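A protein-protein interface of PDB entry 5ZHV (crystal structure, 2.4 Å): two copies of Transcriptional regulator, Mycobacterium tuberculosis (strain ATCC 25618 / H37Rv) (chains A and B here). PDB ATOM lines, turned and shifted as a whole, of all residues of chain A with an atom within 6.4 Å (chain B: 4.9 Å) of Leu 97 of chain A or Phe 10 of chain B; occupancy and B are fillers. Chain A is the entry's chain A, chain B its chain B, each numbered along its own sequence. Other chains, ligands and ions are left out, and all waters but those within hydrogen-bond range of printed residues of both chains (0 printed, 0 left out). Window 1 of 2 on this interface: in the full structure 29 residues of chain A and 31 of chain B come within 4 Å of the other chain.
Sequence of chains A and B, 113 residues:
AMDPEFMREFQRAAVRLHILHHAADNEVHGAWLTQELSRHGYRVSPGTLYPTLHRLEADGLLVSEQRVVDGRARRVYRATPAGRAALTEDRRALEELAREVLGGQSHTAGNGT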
ATOM      1  N   PHE A   6       5.164 -33.904 -15.021  1.00  0.00           N
ATOM      2  CA  PHE A   6       4.837 -32.522 -15.358  1.00  0.00           C
ATOM      3  C   PHE A   6       3.694 -32.470 -16.353  1.00  0.00           C
ATOM      4  O   PHE A   6       2.726 -31.740 -16.115  1.00  0.00           O
ATOM      5  CB  PHE A   6       6.003 -31.732 -15.936  1.00  0.00           C
ATOM      6  CG  PHE A   6       5.618 -30.333 -16.363  1.00  0.00           C
ATOM      7  CD1 PHE A   6       5.136 -30.091 -17.652  1.00  0.00           C
ATOM      8  CD2 PHE A   6       5.690 -29.258 -15.459  1.00  0.00           C
ATOM      9  CE1 PHE A   6       4.759 -28.807 -18.045  1.00  0.00           C
ATOM     10  CE2 PHE A   6       5.304 -27.985 -15.836  1.00  0.00           C
ATOM     11  CZ  PHE A   6       4.841 -27.750 -17.133  1.00  0.00           C
ATOM     12  N   GLU A   9       0.307 -33.516 -14.586  1.00  0.00           N
ATOM     13  CA  GLU A   9      -0.119 -32.396 -13.740  1.00  0.00           C
ATOM     14  C   GLU A   9      -0.567 -31.174 -14.566  1.00  0.00           C
ATOM     15  O   GLU A   9      -1.646 -30.630 -14.323  1.00  0.00           O
ATOM     16  CB  GLU A   9       1.001 -31.981 -12.776  1.00  0.00           C
ATOM     17  CG  GLU A   9       1.424 -33.026 -11.740  1.00  0.00           C
ATOM     18  CD  GLU A   9       2.781 -32.720 -11.086  1.00  0.00           C
ATOM     19  OE1 GLU A   9       3.549 -31.852 -11.591  1.00  0.00           O
ATOM     20  OE2 GLU A   9       3.104 -33.363 -10.047  1.00  0.00           O
ATOM     21  N   PHE A  10       0.249 -30.770 -15.548  1.00  0.00           N
ATOM     22  CA  PHE A  10      -0.016 -29.576 -16.354  1.00  0.00           C
ATOM     23  C   PHE A  10      -1.261 -29.729 -17.226  1.00  0.00           C
ATOM     24  O   PHE A  10      -2.014 -28.757 -17.419  1.00  0.00           O
ATOM     25  CB  PHE A  10       1.181 -29.250 -17.226  1.00  0.00           C
ATOM     26  CG  PHE A  10       1.070 -27.948 -17.979  1.00  0.00           C
ATOM     27  CD1 PHE A  10       1.266 -26.729 -17.334  1.00  0.00           C
ATOM     28  CD2 PHE A  10       0.791 -27.939 -19.351  1.00  0.00           C
ATOM     29  CE1 PHE A  10       1.176 -25.525 -18.042  1.00  0.00           C
ATOM     30  CE2 PHE A  10       0.702 -26.741 -20.063  1.00  0.00           C
ATOM     31  CZ  PHE A  10       0.896 -25.534 -19.410  1.00  0.00           C
ATOM     32  N   ALA A  13      -4.597 -29.093 -15.236  1.00  0.00           N
ATOM     33  CA  ALA A  13      -4.796 -27.660 -15.115  1.00  0.00           C
ATOM     34  C   ALA A  13      -5.228 -27.049 -16.430  1.00  0.00           C
ATOM     35  O   ALA A  13      -6.129 -26.194 -16.455  1.00  0.00           O
ATOM     36  CB  ALA A  13      -3.531 -26.984 -14.607  1.00  0.00           C
ATOM     37  N   ASP A  90      -7.165 -18.264 -12.324  1.00  0.00           N
ATOM     38  CA  ASP A  90      -6.376 -19.308 -12.962  1.00  0.00           C
ATOM     39  C   ASP A  90      -5.486 -18.754 -14.072  1.00  0.00           C
ATOM     40  O   ASP A  90      -4.294 -19.048 -14.095  1.00  0.00           O
ATOM     41  CB  ASP A  90      -7.258 -20.452 -13.482  1.00  0.00           C
ATOM     42  CG  ASP A  90      -8.134 -21.080 -12.389  1.00  0.00           C
ATOM     43  OD1 ASP A  90      -7.947 -20.800 -11.182  1.00  0.00           O
ATOM     44  OD2 ASP A  90      -9.036 -21.860 -12.755  1.00  0.00           O
ATOM     45  N   ARG A  92      -4.416 -15.790 -14.338  1.00  0.00           N
ATOM     46  CA  ARG A  92      -3.418 -14.960 -13.680  1.00  0.00           C
ATOM     47  C   ARG A  92      -2.221 -15.767 -13.162  1.00  0.00           C
ATOM     48  O   ARG A  92      -1.070 -15.381 -13.358  1.00  0.00           O
ATOM     49  CB  ARG A  92      -4.039 -14.098 -12.583  1.00  0.00           C
ATOM     50  CG  ARG A  92      -3.211 -12.840 -12.321  1.00  0.00           C
ATOM     51  CD  ARG A  92      -3.952 -11.777 -11.475  1.00  0.00           C
ATOM     52  NE  ARG A  92      -5.096 -11.122 -12.133  1.00  0.00           N
ATOM     53  N   ALA A  93      -2.513 -16.905 -12.533  1.00  0.00           N
ATOM     54  CA  ALA A  93      -1.501 -17.870 -12.092  1.00  0.00           C
ATOM     55  C   ALA A  93      -0.640 -18.380 -13.259  1.00  0.00           C
ATOM     56  O   ALA A  93       0.574 -18.537 -13.125  1.00  0.00           O
ATOM     57  CB  ALA A  93      -2.154 -19.032 -11.346  1.00  0.00           C
ATOM     58  N   LEU A  94      -1.276 -18.629 -14.400  1.00  0.00           N
ATOM     59  CA  LEU A  94      -0.574 -19.046 -15.610  1.00  0.00           C
ATOM     60  C   LEU A  94       0.379 -17.956 -16.093  1.00  0.00           C
ATOM     61  O   LEU A  94       1.564 -18.240 -16.340  1.00  0.00           O
ATOM     62  CB  LEU A  94      -1.565 -19.423 -16.708  1.00  0.00           C
ATOM     63  CG  LEU A  94      -1.102 -19.833 -18.115  1.00  0.00           C
ATOM     64  CD1 LEU A  94      -0.253 -21.094 -18.099  1.00  0.00           C
ATOM     65  CD2 LEU A  94      -2.317 -20.082 -18.997  1.00  0.00           C
ATOM     66  N   GLU A  95      -0.138 -16.733 -16.209  1.00  0.00           N
ATOM     67  CA  GLU A  95       0.653 -15.575 -16.629  1.00  0.00           C
ATOM     68  C   GLU A  95       1.903 -15.398 -15.741  1.00  0.00           C
ATOM     69  O   GLU A  95       3.007 -15.185 -16.250  1.00  0.00           O
ATOM     70  CB  GLU A  95      -0.157 -14.276 -16.615  1.00  0.00           C
ATOM     71  CG  GLU A  95      -1.426 -14.245 -17.461  1.00  0.00           C
ATOM     72  CD  GLU A  95      -2.123 -12.880 -17.435  1.00  0.00           C
ATOM     73  OE1 GLU A  95      -3.288 -12.805 -16.982  1.00  0.00           O
ATOM     74  OE2 GLU A  95      -1.526 -11.870 -17.889  1.00  0.00           O
ATOM     75  N   GLU A  96       1.700 -15.515 -14.427  1.00  0.00           N
ATOM     76  CA  GLU A  96       2.760 -15.365 -13.447  1.00  0.00           C
ATOM     77  C   GLU A  96       3.876 -16.374 -13.722  1.00  0.00           C
ATOM     78  O   GLU A  96       5.028 -15.989 -13.852  1.00  0.00           O
ATOM     79  CB  GLU A  96       2.205 -15.489 -12.026  1.00  0.00           C
ATOM     80  CG  GLU A  96       3.153 -15.097 -10.892  1.00  0.00           C
ATOM     81  N   LEU A  97       3.512 -17.649 -13.863  1.00  0.00           N
ATOM     82  CA  LEU A  97       4.477 -18.729 -14.078  1.00  0.00           C
ATOM     83  C   LEU A  97       5.167 -18.598 -15.441  1.00  0.00           C
ATOM     84  O   LEU A  97       6.359 -18.860 -15.551  1.00  0.00           O
ATOM     85  CB  LEU A  97       3.822 -20.096 -13.914  1.00  0.00           C
ATOM     86  CG  LEU A  97       4.792 -21.289 -14.036  1.00  0.00           C
ATOM     87  CD1 LEU A  97       5.906 -21.278 -12.984  1.00  0.00           C
ATOM     88  CD2 LEU A  97       4.078 -22.631 -14.081  1.00  0.00           C
ATOM     89  N   ALA A  98       4.418 -18.181 -16.455  1.00  0.00           N
ATOM     90  CA  ALA A  98       4.993 -17.804 -17.769  1.00  0.00           C
ATOM     91  C   ALA A  98       6.056 -16.705 -17.654  1.00  0.00           C
ATOM     92  O   ALA A  98       7.169 -16.878 -18.175  1.00  0.00           O
ATOM     93  CB  ALA A  98       3.912 -17.390 -18.755  1.00  0.00           C
ATOM     94  N   ARG A  99       5.723 -15.611 -16.957  1.00  0.00           N
ATOM     95  CA  ARG A  99       6.673 -14.520 -16.688  1.00  0.00           C
ATOM     96  C   ARG A  99       7.965 -14.998 -15.999  1.00  0.00           C
ATOM     97  O   ARG A  99       9.052 -14.589 -16.359  1.00  0.00           O
ATOM     98  CB  ARG A  99       6.013 -13.418 -15.836  1.00  0.00           C
ATOM     99  CG  ARG A  99       5.674 -12.116 -16.529  1.00  0.00           C
ATOM    100  CD  ARG A  99       5.315 -11.013 -15.531  1.00  0.00           C
ATOM    101  NE  ARG A  99       4.788 -11.434 -14.224  1.00  0.00           N
ATOM    102  CZ  ARG A  99       3.499 -11.548 -13.893  1.00  0.00           C
ATOM    103  NH1 ARG A  99       2.535 -11.248 -14.764  1.00  0.00           N
ATOM    104  NH2 ARG A  99       3.162 -11.958 -12.663  1.00  0.00           N
ATOM    105  N   GLU A 100       7.815 -15.881 -15.022  1.00  0.00           N
ATOM    106  CA  GLU A 100       8.908 -16.366 -14.181  1.00  0.00           C
ATOM    107  C   GLU A 100       9.950 -17.217 -14.927  1.00  0.00           C
ATOM    108  O   GLU A 100      11.163 -17.008 -14.774  1.00  0.00           O
ATOM    109  CB  GLU A 100       8.333 -17.163 -12.999  1.00  0.00           C
ATOM    110  CG  GLU A 100       8.039 -16.363 -11.727  1.00  0.00           C
ATOM    111  CD  GLU A 100       6.892 -16.932 -10.907  1.00  0.00           C
ATOM    112  OE1 GLU A 100       6.463 -18.078 -11.166  1.00  0.00           O
ATOM    113  OE2 GLU A 100       6.405 -16.222  -9.997  1.00  0.00           O
ATOM    114  N   VAL A 101       9.487 -18.182 -15.726  1.00  0.00           N
ATOM    115  CA  VAL A 101      10.400 -19.222 -16.251  1.00  0.00           C
ATOM    116  C   VAL A 101      10.722 -19.097 -17.736  1.00  0.00           C
ATOM    117  O   VAL A 101      11.550 -19.848 -18.253  1.00  0.00           O
ATOM    118  CB  VAL A 101       9.979 -20.675 -15.876  1.00  0.00           C
ATOM    119  CG1 VAL A 101       9.887 -20.839 -14.372  1.00  0.00           C
ATOM    120  CG2 VAL A 101       8.671 -21.076 -16.536  1.00  0.00           C
ATOM    121  N   LEU A 102      10.095 -18.133 -18.403  1.00  0.00           N
ATOM    122  CA  LEU A 102      10.413 -17.808 -19.793  1.00  0.00           C
ATOM    123  C   LEU A 102      11.224 -16.491 -19.964  1.00  0.00           C
ATOM    124  O   LEU A 102      11.603 -15.817 -19.001  1.00  0.00           O
ATOM    125  CB  LEU A 102       9.141 -17.851 -20.656  1.00  0.00           C
ATOM    126  CG  LEU A 102       8.159 -19.030 -20.460  1.00  0.00           C
ATOM    127  CD1 LEU A 102       6.854 -18.837 -21.212  1.00  0.00           C
ATOM    128  CD2 LEU A 102       8.776 -20.362 -20.831  1.00  0.00           C
ATOM    129  N   GLU B   5      -8.704 -26.378  -6.489  1.00  0.00           N
ATOM    130  CA  GLU B   5      -8.241 -27.565  -7.212  1.00  0.00           C
ATOM    131  C   GLU B   5      -7.284 -27.190  -8.359  1.00  0.00           C
ATOM    132  O   GLU B   5      -6.230 -27.815  -8.510  1.00  0.00           O
ATOM    133  CB  GLU B   5      -9.425 -28.440  -7.686  1.00  0.00           C
ATOM    134  CG  GLU B   5      -9.049 -29.826  -8.216  1.00  0.00           C
ATOM    135  CD  GLU B   5      -8.266 -30.680  -7.213  1.00  0.00           C
ATOM    136  OE2 GLU B   5      -7.265 -31.346  -7.588  1.00  0.00           O
ATOM    137  N   PHE B   6      -7.631 -26.155  -9.128  1.00  0.00           N
ATOM    138  CA  PHE B   6      -6.701 -25.626 -10.124  1.00  0.00           C
ATOM    139  C   PHE B   6      -5.402 -25.193  -9.472  1.00  0.00           C
ATOM    140  O   PHE B   6      -4.343 -25.600  -9.934  1.00  0.00           O
ATOM    141  CB  PHE B   6      -7.254 -24.447 -10.911  1.00  0.00           C
ATOM    142  CG  PHE B   6      -6.248 -23.843 -11.863  1.00  0.00           C
ATOM    143  CD1 PHE B   6      -5.360 -22.840 -11.441  1.00  0.00           C
ATOM    144  CD2 PHE B   6      -6.171 -24.294 -13.182  1.00  0.00           C
ATOM    145  CE1 PHE B   6      -4.418 -22.310 -12.314  1.00  0.00           C
ATOM    146  CE2 PHE B   6      -5.249 -23.754 -14.070  1.00  0.00           C
ATOM    147  CZ  PHE B   6      -4.364 -22.766 -13.628  1.00  0.00           C
ATOM    148  N   MET B   7      -5.482 -24.371  -8.422  1.00  0.00           N
ATOM    149  CA  MET B   7      -4.279 -23.873  -7.745  1.00  0.00           C
ATOM    150  C   MET B   7      -3.377 -24.991  -7.228  1.00  0.00           C
ATOM    151  O   MET B   7      -2.153 -24.936  -7.377  1.00  0.00           O
ATOM    152  CB  MET B   7      -4.602 -22.855  -6.644  1.00  0.00           C
ATOM    153  CG  MET B   7      -5.169 -21.543  -7.156  1.00  0.00           C
ATOM    154  SD  MET B   7      -4.156 -20.656  -8.385  1.00  0.00           S
ATOM    155  CE  MET B   7      -5.277 -19.311  -8.792  1.00  0.00           C
ATOM    156  N   ARG B   8      -4.009 -26.018  -6.670  1.00  0.00           N
ATOM    157  CA  ARG B   8      -3.337 -27.190  -6.138  1.00  0.00           C
ATOM    158  C   ARG B   8      -2.612 -27.965  -7.257  1.00  0.00           C
ATOM    159  O   ARG B   8      -1.378 -28.148  -7.194  1.00  0.00           O
ATOM    160  CB  ARG B   8      -4.381 -28.040  -5.411  1.00  0.00           C
ATOM    161  CG  ARG B   8      -3.892 -29.284  -4.686  1.00  0.00           C
ATOM    162  CD  ARG B   8      -4.901 -29.725  -3.624  1.00  0.00           C
ATOM    163  NE  ARG B   8      -6.273 -29.917  -4.119  1.00  0.00           N
ATOM    164  CZ  ARG B   8      -7.334 -29.177  -3.770  1.00  0.00           C
ATOM    165  NH1 ARG B   8      -7.241 -28.156  -2.918  1.00  0.00           N
ATOM    166  NH2 ARG B   8      -8.536 -29.468  -4.260  1.00  0.00           N
ATOM    167  N   GLU B   9      -3.361 -28.372  -8.285  1.00  0.00           N
ATOM    168  CA  GLU B   9      -2.783 -29.005  -9.475  1.00  0.00           C
ATOM    169  C   GLU B   9      -1.681 -28.154 -10.115  1.00  0.00           C
ATOM    170  O   GLU B   9      -0.585 -28.661 -10.396  1.00  0.00           O
ATOM    171  CB  GLU B   9      -3.866 -29.297 -10.523  1.00  0.00           C
ATOM    172  CG  GLU B   9      -4.940 -30.312 -10.124  1.00  0.00           C
ATOM    173  CD  GLU B   9      -6.186 -30.257 -11.019  1.00  0.00           C
ATOM    174  OE1 GLU B   9      -6.337 -29.279 -11.809  1.00  0.00           O
ATOM    175  OE2 GLU B   9      -7.027 -31.197 -10.936  1.00  0.00           O
ATOM    176  N   PHE B  10      -1.964 -26.865 -10.324  1.00  0.00           N
ATOM    177  CA  PHE B  10      -1.042 -25.959 -11.012  1.00  0.00           C
ATOM    178  C   PHE B  10       0.238 -25.721 -10.226  1.00  0.00           C
ATOM    179  O   PHE B  10       1.310 -25.609 -10.816  1.00  0.00           O
ATOM    180  CB  PHE B  10      -1.715 -24.624 -11.307  1.00  0.00           C
ATOM    181  CG  PHE B  10      -0.907 -23.718 -12.186  1.00  0.00           C
ATOM    182  CD1 PHE B  10      -0.819 -23.951 -13.564  1.00  0.00           C
ATOM    183  CD2 PHE B  10      -0.255 -22.610 -11.652  1.00  0.00           C
ATOM    184  CE1 PHE B  10      -0.063 -23.120 -14.381  1.00  0.00           C
ATOM    185  CE2 PHE B  10       0.496 -21.761 -12.461  1.00  0.00           C
ATOM    186  CZ  PHE B  10       0.587 -22.019 -13.827  1.00  0.00           C
ATOM    187  N   GLN B  11       0.119 -25.635  -8.907  1.00  0.00           N
ATOM    188  CA  GLN B  11       1.289 -25.457  -8.078  1.00  0.00           C
ATOM    189  C   GLN B  11       2.288 -26.626  -8.171  1.00  0.00           C
ATOM    190  O   GLN B  11       3.486 -26.384  -8.228  1.00  0.00           O
ATOM    191  CB  GLN B  11       0.943 -25.099  -6.628  1.00  0.00           C
ATOM    192  CG  GLN B  11       2.155 -24.467  -5.954  1.00  0.00           C
ATOM    193  CD  GLN B  11       1.902 -23.931  -4.570  1.00  0.00           C
ATOM    194  OE1 GLN B  11       1.352 -22.827  -4.394  1.00  0.00           O
ATOM    195  NE2 GLN B  11       2.334 -24.692  -3.568  1.00  0.00           N
ATOM    196  N   ARG B  12       1.792 -27.865  -8.215  1.00  0.00           N
ATOM    197  CA  ARG B  12       2.657 -29.052  -8.327  1.00  0.00           C
ATOM    198  C   ARG B  12       3.545 -28.928  -9.564  1.00  0.00           C
ATOM    199  O   ARG B  12       4.785 -29.059  -9.495  1.00  0.00           O
ATOM    200  CB  ARG B  12       1.837 -30.342  -8.377  1.00  0.00           C
ATOM    201  CG  ARG B  12       1.271 -30.795  -7.045  1.00  0.00           C
ATOM    202  CD  ARG B  12       0.839 -32.261  -7.057  1.00  0.00           C
ATOM    203  NE  ARG B  12      -0.506 -32.389  -7.629  1.00  0.00           N
ATOM    204  CZ  ARG B  12      -1.665 -32.266  -6.956  1.00  0.00           C
ATOM    205  NH1 ARG B  12      -1.690 -32.037  -5.636  1.00  0.00           N
ATOM    206  NH2 ARG B  12      -2.822 -32.379  -7.617  1.00  0.00           N
ATOM    207  N   ALA B  13       2.897 -28.606 -10.682  1.00  0.00           N
ATOM    208  CA  ALA B  13       3.579 -28.411 -11.951  1.00  0.00           C
ATOM    209  C   ALA B  13       4.537 -27.240 -11.885  1.00  0.00           C
ATOM    210  O   ALA B  13       5.668 -27.330 -12.405  1.00  0.00           O
ATOM    211  CB  ALA B  13       2.561 -28.198 -13.067  1.00  0.00           C
ATOM    212  N   ALA B  14       4.088 -26.149 -11.265  1.00  0.00           N
ATOM    213  CA  ALA B  14       4.895 -24.946 -11.146  1.00  0.00           C
ATOM    214  C   ALA B  14       6.194 -25.192 -10.354  1.00  0.00           C
ATOM    215  O   ALA B  14       7.268 -24.728 -10.746  1.00  0.00           O
ATOM    216  CB  ALA B  14       4.085 -23.836 -10.491  1.00  0.00           C
ATOM    217  N   LEU B  17       8.625 -27.429 -12.356  1.00  0.00           N
ATOM    218  CA  LEU B  17       9.269 -26.577 -13.336  1.00  0.00           C
ATOM    219  C   LEU B  17      10.344 -25.661 -12.734  1.00  0.00           C
ATOM    220  O   LEU B  17      11.427 -25.502 -13.321  1.00  0.00           O
ATOM    221  CB  LEU B  17       8.215 -25.751 -14.037  1.00  0.00           C
ATOM    222  CG  LEU B  17       8.509 -25.066 -15.368  1.00  0.00           C
ATOM    223  CD1 LEU B  17       9.118 -25.984 -16.391  1.00  0.00           C
ATOM    224  CD2 LEU B  17       7.217 -24.533 -15.929  1.00  0.00           C
ATOM    225  N   HIS B  18      10.040 -25.045 -11.582  1.00  0.00           N
ATOM    226  CA  HIS B  18      10.992 -24.138 -10.930  1.00  0.00           C
ATOM    227  C   HIS B  18      12.225 -24.870 -10.434  1.00  0.00           C
ATOM    228  O   HIS B  18      13.317 -24.337 -10.513  1.00  0.00           O
ATOM    229  CB  HIS B  18      10.362 -23.352  -9.791  1.00  0.00           C
ATOM    230  CG  HIS B  18       9.798 -22.033 -10.202  1.00  0.00           C
ATOM    231  ND1 HIS B  18      10.574 -20.903 -10.393  1.00  0.00           N
ATOM    232  CD2 HIS B  18       8.523 -21.662 -10.477  1.00  0.00           C
ATOM    233  CE1 HIS B  18       9.798 -19.901 -10.773  1.00  0.00           C
ATOM    234  NE2 HIS B  18       8.548 -20.332 -10.826  1.00  0.00           N
ATOM    235  N   TYR B  42       5.722 -19.448  -3.859  1.00  0.00           N
ATOM    236  CA  TYR B  42       5.168 -20.795  -3.662  1.00  0.00           C
ATOM    237  C   TYR B  42       5.405 -21.289  -2.245  1.00  0.00           C
ATOM    238  O   TYR B  42       6.537 -21.317  -1.779  1.00  0.00           O
ATOM    239  CB  TYR B  42       5.698 -21.778  -4.734  1.00  0.00           C
ATOM    240  CG  TYR B  42       5.436 -21.316  -6.160  1.00  0.00           C
ATOM    241  CD1 TYR B  42       4.198 -21.547  -6.782  1.00  0.00           C
ATOM    242  CD2 TYR B  42       6.409 -20.614  -6.878  1.00  0.00           C
ATOM    243  CE1 TYR B  42       3.930 -21.090  -8.071  1.00  0.00           C
ATOM    244  CE2 TYR B  42       6.166 -20.152  -8.171  1.00  0.00           C
ATOM    245  CZ  TYR B  42       4.928 -20.409  -8.773  1.00  0.00           C
ATOM    246  OH  TYR B  42       4.699 -19.964 -10.061  1.00  0.00           O
ATOM    247  N   LEU B  94       4.063 -24.678 -21.487  1.00  0.00           N
ATOM    248  CA  LEU B  94       3.660 -23.482 -20.770  1.00  0.00           C
ATOM    249  C   LEU B  94       3.456 -22.329 -21.730  1.00  0.00           C
ATOM    250  O   LEU B  94       2.403 -21.686 -21.703  1.00  0.00           O
ATOM    251  CB  LEU B  94       4.703 -23.095 -19.706  1.00  0.00           C
ATOM    252  CG  LEU B  94       4.502 -21.839 -18.832  1.00  0.00           C
ATOM    253  CD1 LEU B  94       3.258 -21.924 -17.976  1.00  0.00           C
ATOM    254  CD2 LEU B  94       5.697 -21.611 -17.936  1.00  0.00           C
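Printed residues of chain B within 4 Å of Leu 97 of chain A: Phe 10 (3.6 Å), Ala 14 (3.8 Å), His 18 (3.5 Å), Tyr 42 (3.4 Å) and Leu 94 (3.7 Å). Phe 10 of chain B touches three residues of chain A. Of the printed residues of chain B, Phe 10 of chain A touches Leu 94 (3.7 Å). Printed residues of chain A within 4 Å of Tyr 42 of chain B: Leu 97 and Glu 100. The nearest printed residue of chain B that does not touch Leu 94 of chain A is Phe 6 of chain B (5.2 Å).
Hydrophobic or aromatic side chains of chain A that line the printed part of chain B: Phe 6, Phe 10, Ala 13, Ala 93, Leu 94, Leu 97 and Val 101. Of the 14 printed residues of chain B, 11 touch a printed residue of chain A. Among the printed residues, 24 pairs touch across the chains.
Among the printed residues, merely in contact across the chains: Phe 6 of chain A with Ala 13 of chain B (3.5 Å), Phe 6 of chain A with Leu 17 of chain B (3.9 Å), Glu 9 of chain A with Arg 12 of chain B (3.6 Å), Phe 10 of chain A with Leu 94 of chain B (3.7 Å), Ala 13 of chain A with Phe 6 of chain B (3.5 Å), Ala 13 of chain A with Glu 9 of chain B (3.8 Å), Asp 90 of chain A with Phe 6 of chain B (3.3 Å), Asp 90 of chain A with Met 7 of chain B (3.9 Å), Ala 93 of chain A with Met 7 of chain B (3.9 Å), Ala 93 of chain A with Phe 10 of chain B (3.3 Å), Leu 94 of chain A with Phe 10 of chain B (3.7 Å), Leu 94 of chain A with Leu 94 of chain B (3.6 Å), Leu 97 of chain A with Phe 10 of chain B (3.6 Å), Leu 97 of chain A with Ala 14 of chain B (3.8 Å), Leu 97 of chain A with His 18 of chain B (3.5 Å), Leu 97 of chain A with Tyr 42 of chain B (3.4 Å), Leu 97 of chain A with Leu 94 of chain B (3.7 Å), Ala 98 of chain A with Leu 94 of chain B (3.9 Å), Val 101 of chain A with Leu 17 of chain B (3.8 Å), Val 101 of chain A with His 18 of chain B (3.7 Å) and Val 101 of chain A with Leu 94 of chain B (3.3 Å).
The backbone NH (N) of Ala 13 of chain B sits at hydrogen-bond distance from the side-chain carboxylate (OE1) of Glu 9 of chain A, at 3.4 Å. The side-chain carboxylate (OE1) of Glu 100 of chain A sits at hydrogen-bond distance from a ring nitrogen (NE2) of His 18 of chain B. OE1 of Glu 100 of chain A lies within hydrogen-bond range of OH of Tyr 42 of chain B.
Phe 6 of chain A touches Ala 13 of chain B, and with the chains exchanged Ala 13 of chain A touches Phe 6 of chain B. Glu 9 of chain A touches Ala 13 of chain B, and with the chains exchanged Ala 13 of chain A touches Glu 9 of chain B. Phe 10 of chain A touches Leu 94 of chain B, and with the chains exchanged Leu 94 of chain A touches Phe 10 of chain B. Leu 94 of chain A touches its own counterpart, Leu 94 of chain B. Positions printed for both chains: 6, 9, 10, 13 and 94. Of the 24 pairs that touch across the chains among the printed residues, 7 have their exchanged pair printed and touching as well.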
